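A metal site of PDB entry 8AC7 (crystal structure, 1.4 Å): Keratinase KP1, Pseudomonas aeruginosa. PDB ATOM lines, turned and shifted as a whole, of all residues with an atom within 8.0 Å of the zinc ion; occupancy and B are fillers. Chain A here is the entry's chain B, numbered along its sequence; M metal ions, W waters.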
ATOM      1  N   ILE A 354     -14.380  18.134 -21.990  1.00  0.00           N
ATOM      2  CA  ILE A 354     -15.311  18.924 -21.195  1.00  0.00           C
ATOM      3  C   ILE A 354     -15.627  20.183 -21.990  1.00  0.00           C
ATOM      4  O   ILE A 354     -14.713  20.854 -22.480  1.00  0.00           O
ATOM      5  CB  ILE A 354     -14.702  19.279 -19.822  1.00  0.00           C
ATOM      6  CG1 ILE A 354     -14.422  18.009 -19.019  1.00  0.00           C
ATOM      7  CG2 ILE A 354     -15.615  20.247 -19.062  1.00  0.00           C
ATOM      8  CD1 ILE A 354     -13.593  18.250 -17.753  1.00  0.00           C
ATOM      9  N   TYR A 355     -16.912  20.527 -22.107  1.00  0.00           N
ATOM     10  CA  TYR A 355     -17.282  21.713 -22.861  1.00  0.00           C
ATOM     11  C   TYR A 355     -16.510  22.926 -22.346  1.00  0.00           C
ATOM     12  O   TYR A 355     -16.443  23.177 -21.145  1.00  0.00           O
ATOM     13  CB  TYR A 355     -18.782  21.988 -22.724  1.00  0.00           C
ATOM     14  CG  TYR A 355     -19.720  21.035 -23.449  1.00  0.00           C
ATOM     15  CD1 TYR A 355     -21.085  21.282 -23.461  1.00  0.00           C
ATOM     16  CD2 TYR A 355     -19.254  19.898 -24.109  1.00  0.00           C
ATOM     17  CE1 TYR A 355     -21.952  20.450 -24.088  1.00  0.00           C
ATOM     18  CE2 TYR A 355     -20.136  19.048 -24.758  1.00  0.00           C
ATOM     19  CZ  TYR A 355     -21.482  19.335 -24.733  1.00  0.00           C
ATOM     20  OH  TYR A 355     -22.395  18.512 -25.362  1.00  0.00           O
ATOM     21  N   ASP A 356     -15.948  23.701 -23.282  1.00  0.00           N
ATOM     22  CA  ASP A 356     -15.077  24.834 -22.947  1.00  0.00           C
ATOM     23  C   ASP A 356     -15.894  26.105 -22.687  1.00  0.00           C
ATOM     24  O   ASP A 356     -15.797  27.112 -23.383  1.00  0.00           O
ATOM     25  CB  ASP A 356     -14.077  25.031 -24.095  1.00  0.00           C
ATOM     26  CG  ASP A 356     -13.104  26.154 -23.841  1.00  0.00           C
ATOM     27  OD1 ASP A 356     -12.674  26.355 -22.696  1.00  0.00           O
ATOM     28  OD2 ASP A 356     -12.724  26.830 -24.821  1.00  0.00           O
ATOM     29  N   GLY A 357     -16.709  26.050 -21.619  1.00  0.00           N
ATOM     30  CA  GLY A 357     -17.618  27.144 -21.311  1.00  0.00           C
ATOM     31  C   GLY A 357     -16.949  28.467 -21.005  1.00  0.00           C
ATOM     32  O   GLY A 357     -17.559  29.532 -21.152  1.00  0.00           O
ATOM     33  N   ASP A 358     -15.698  28.438 -20.535  1.00  0.00           N
ATOM     34  CA  ASP A 358     -14.963  29.661 -20.238  1.00  0.00           C
ATOM     35  C   ASP A 358     -14.173  30.186 -21.437  1.00  0.00           C
ATOM     36  O   ASP A 358     -13.481  31.197 -21.298  1.00  0.00           O
ATOM     37  CB  ASP A 358     -14.034  29.489 -19.027  1.00  0.00           C
ATOM     38  CG  ASP A 358     -12.948  28.447 -19.224  1.00  0.00           C
ATOM     39  OD1 ASP A 358     -12.818  27.891 -20.343  1.00  0.00           O
ATOM     40  OD2 ASP A 358     -12.207  28.179 -18.256  1.00  0.00           O
ATOM     41  N   GLY A 359     -14.264  29.530 -22.589  1.00  0.00           N
ATOM     42  CA  GLY A 359     -13.535  29.993 -23.761  1.00  0.00           C
ATOM     43  C   GLY A 359     -12.023  29.891 -23.675  1.00  0.00           C
ATOM     44  O   GLY A 359     -11.335  30.469 -24.519  1.00  0.00           O
ATOM     45  N   SER A 360     -11.492  29.170 -22.676  1.00  0.00           N
ATOM     46  CA  SER A 360     -10.052  29.113 -22.467  1.00  0.00           C
ATOM     47  C   SER A 360      -9.305  28.506 -23.656  1.00  0.00           C
ATOM     48  O   SER A 360      -8.145  28.852 -23.898  1.00  0.00           O
ATOM     49  CB  SER A 360      -9.741  28.319 -21.193  1.00  0.00           C
ATOM     50  OG  SER A 360     -10.180  26.961 -21.300  1.00  0.00           O
ATOM     51  N   ASP A 361      -9.949  27.598 -24.395  1.00  0.00           N
ATOM     52  CA  ASP A 361      -9.312  26.917 -25.518  1.00  0.00           C
ATOM     53  C   ASP A 361      -9.676  27.517 -26.863  1.00  0.00           C
ATOM     54  O   ASP A 361      -8.793  27.719 -27.708  1.00  0.00           O
ATOM     55  CB  ASP A 361      -9.701  25.436 -25.534  1.00  0.00           C
ATOM     56  CG  ASP A 361      -9.210  24.682 -24.306  1.00  0.00           C
ATOM     57  OD1 ASP A 361      -8.027  24.805 -23.951  1.00  0.00           O
ATOM     58  OD2 ASP A 361     -10.040  23.972 -23.692  1.00  0.00           O
ATOM     59  N   PHE A 362     -10.951  27.810 -27.085  1.00  0.00           N
ATOM     60  CA  PHE A 362     -11.436  28.172 -28.400  1.00  0.00           C
ATOM     61  C   PHE A 362     -12.036  29.573 -28.494  1.00  0.00           C
ATOM     62  O   PHE A 362     -12.516  29.951 -29.573  1.00  0.00           O
ATOM     63  CB  PHE A 362     -12.417  27.106 -28.918  1.00  0.00           C
ATOM     64  CG  PHE A 362     -11.920  25.703 -28.737  1.00  0.00           C
ATOM     65  CD1 PHE A 362     -12.444  24.894 -27.737  1.00  0.00           C
ATOM     66  CD2 PHE A 362     -10.908  25.194 -29.540  1.00  0.00           C
ATOM     67  CE1 PHE A 362     -11.978  23.601 -27.557  1.00  0.00           C
ATOM     68  CE2 PHE A 362     -10.437  23.905 -29.367  1.00  0.00           C
ATOM     69  CZ  PHE A 362     -10.983  23.106 -28.364  1.00  0.00           C
ATOM     70  N   GLY A 363     -12.023  30.359 -27.423  1.00  0.00           N
ATOM     71  CA  GLY A 363     -12.428  31.751 -27.470  1.00  0.00           C
ATOM     72  C   GLY A 363     -13.919  32.017 -27.484  1.00  0.00           C
ATOM     73  O   GLY A 363     -14.315  33.183 -27.547  1.00  0.00           O
ATOM     74  N   LEU A 364     -14.763  30.995 -27.426  1.00  0.00           N
ATOM     75  CA  LEU A 364     -16.203  31.164 -27.361  1.00  0.00           C
ATOM     76  C   LEU A 364     -16.657  30.860 -25.941  1.00  0.00           C
ATOM     77  O   LEU A 364     -16.444  29.747 -25.444  1.00  0.00           O
ATOM     78  CB  LEU A 364     -16.907  30.234 -28.353  1.00  0.00           C
ATOM     79  CG  LEU A 364     -18.436  30.310 -28.411  1.00  0.00           C
ATOM     80  CD1 LEU A 364     -18.916  31.720 -28.728  1.00  0.00           C
ATOM     81  CD2 LEU A 364     -18.996  29.314 -29.414  1.00  0.00           C
ATOM     82  N   SER A 370     -21.454  29.301 -17.029  1.00  0.00           N
ATOM     83  CA  SER A 370     -20.891  28.201 -17.801  1.00  0.00           C
ATOM     84  C   SER A 370     -19.457  27.899 -17.365  1.00  0.00           C
ATOM     85  O   SER A 370     -19.043  26.728 -17.361  1.00  0.00           O
ATOM     86  CB  SER A 370     -20.927  28.557 -19.289  1.00  0.00           C
ATOM     87  OG  SER A 370     -22.255  28.748 -19.738  1.00  0.00           O
ATOM     88  N   ALA A 371     -18.691  28.919 -16.997  1.00  0.00           N
ATOM     89  CA  ALA A 371     -17.336  28.670 -16.520  1.00  0.00           C
ATOM     90  C   ALA A 371     -17.340  27.854 -15.236  1.00  0.00           C
ATOM     91  O   ALA A 371     -16.550  26.916 -15.085  1.00  0.00           O
ATOM     92  CB  ALA A 371     -16.585  29.988 -16.336  1.00  0.00           C
ATOM     93  N   GLU A 374     -18.061  24.155 -16.077  1.00  0.00           N
ATOM     94  CA  GLU A 374     -16.846  23.550 -16.614  1.00  0.00           C
ATOM     95  C   GLU A 374     -15.845  23.250 -15.507  1.00  0.00           C
ATOM     96  O   GLU A 374     -15.231  22.171 -15.490  1.00  0.00           O
ATOM     97  CB  GLU A 374     -16.244  24.503 -17.650  1.00  0.00           C
ATOM     98  CG  GLU A 374     -14.951  24.041 -18.293  1.00  0.00           C
ATOM     99  CD  GLU A 374     -14.342  25.116 -19.183  1.00  0.00           C
ATOM    100  OE1 GLU A 374     -14.749  26.281 -19.045  1.00  0.00           O
ATOM    101  OE2 GLU A 374     -13.457  24.794 -20.014  1.00  0.00           O
ATOM    102  N   ARG A 375     -15.675  24.194 -14.583  1.00  0.00           N
ATOM    103  CA  ARG A 375     -14.706  24.031 -13.504  1.00  0.00           C
ATOM    104  C   ARG A 375     -15.090  22.851 -12.600  1.00  0.00           C
ATOM    105  O   ARG A 375     -14.207  22.120 -12.131  1.00  0.00           O
ATOM    106  CB  ARG A 375     -14.617  25.332 -12.710  1.00  0.00           C
ATOM    107  CG  ARG A 375     -13.440  25.410 -11.746  1.00  0.00           C
ATOM    108  CD  ARG A 375     -13.272  26.844 -11.231  1.00  0.00           C
ATOM    109  NE  ARG A 375     -13.070  27.793 -12.327  1.00  0.00           N
ATOM    110  CZ  ARG A 375     -13.949  28.733 -12.684  1.00  0.00           C
ATOM    111  NH1 ARG A 375     -15.096  28.848 -12.036  1.00  0.00           N
ATOM    112  NH2 ARG A 375     -13.663  29.556 -13.692  1.00  0.00           N
ATOM    113  N   GLU A 378     -14.028  19.806 -14.526  1.00  0.00           N
ATOM    114  CA  GLU A 378     -12.573  19.728 -14.512  1.00  0.00           C
ATOM    115  C   GLU A 378     -12.059  19.250 -13.160  1.00  0.00           C
ATOM    116  O   GLU A 378     -11.177  18.388 -13.088  1.00  0.00           O
ATOM    117  CB  GLU A 378     -11.963  21.096 -14.839  1.00  0.00           C
ATOM    118  CG  GLU A 378     -12.169  21.533 -16.284  1.00  0.00           C
ATOM    119  CD  GLU A 378     -11.772  22.987 -16.528  1.00  0.00           C
ATOM    120  OE1 GLU A 378     -11.574  23.363 -17.699  1.00  0.00           O
ATOM    121  OE2 GLU A 378     -11.658  23.763 -15.551  1.00  0.00           O
ATOM    122  N   GLU A 389      -9.580  17.805 -21.238  1.00  0.00           N
ATOM    123  CA  GLU A 389      -9.275  18.984 -22.049  1.00  0.00           C
ATOM    124  C   GLU A 389     -10.570  19.517 -22.632  1.00  0.00           C
ATOM    125  O   GLU A 389     -11.610  18.861 -22.593  1.00  0.00           O
ATOM    126  CB  GLU A 389      -8.263  18.670 -23.154  1.00  0.00           C
ATOM    127  CG  GLU A 389      -8.801  17.745 -24.238  1.00  0.00           C
ATOM    128  CD  GLU A 389      -7.680  17.215 -25.109  1.00  0.00           C
ATOM    129  OE1 GLU A 389      -6.966  16.295 -24.658  1.00  0.00           O
ATOM    130  OE2 GLU A 389      -7.506  17.733 -26.229  1.00  0.00           O
ATOM    131  N   GLY A 390     -10.499  20.730 -23.171  1.00  0.00           N
ATOM    132  CA  GLY A 390     -11.678  21.378 -23.681  1.00  0.00           C
ATOM    133  C   GLY A 390     -12.131  20.855 -25.033  1.00  0.00           C
ATOM    134  O   GLY A 390     -11.366  20.281 -25.814  1.00  0.00           O
ATOM    135  N   THR A 391     -13.419  21.043 -25.300  1.00  0.00           N
ATOM    136  CA  THR A 391     -13.974  20.807 -26.630  1.00  0.00           C
ATOM    137  C   THR A 391     -14.890  21.980 -26.976  1.00  0.00           C
ATOM    138  O   THR A 391     -15.390  22.682 -26.098  1.00  0.00           O
ATOM    139  CB  THR A 391     -14.705  19.461 -26.704  1.00  0.00           C
ATOM    140  OG1 THR A 391     -14.980  19.138 -28.080  1.00  0.00           O
ATOM    141  CG2 THR A 391     -16.016  19.499 -25.936  1.00  0.00           C
HETATM  142 ZN    ZN M   1     -12.020  26.028 -20.772  1.00  0.00          ZN
HETATM  143  O   HOH W   1     -11.012  24.317 -21.340  1.00  0.00           O
HETATM  144  O   HOH W   2     -11.095  25.875 -18.733  1.00  0.00           O
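OE1 of Glu 374 lies within hydrogen-bond range of N of Gly 357 (3.2 Å). The side-chain carboxylate of Asp 356 is in hydrogen-bond range of the backbone NH of Asp 361, at 2.9 Å. OD2 of Asp 356 is in hydrogen-bond range of N of Phe 362, 3.0 Å away. N of Asp 356 sits at hydrogen-bond distance from O of Thr 391, at 3.0 Å.
The zinc ion is bound by OE2 of Glu 374 (2.0 Å), OD1 of Asp 356 (2.1 Å), water W1 (2.1 Å), OD1 of Asp 358 (2.1 Å), OG of Ser 360 (2.1 Å) and water W2 (2.2 Å). The zinc ion has six donor atoms within binding distance.
Water W2 bridges OD2 of Asp 358 and OE1 of Glu 378.
Within 4 Å of the zinc ion: Asp 356, Asp 358, Ser 360 and Glu 374. The nearest printed residue that does not touch the zinc ion is Asp 361 (4.1 Å).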
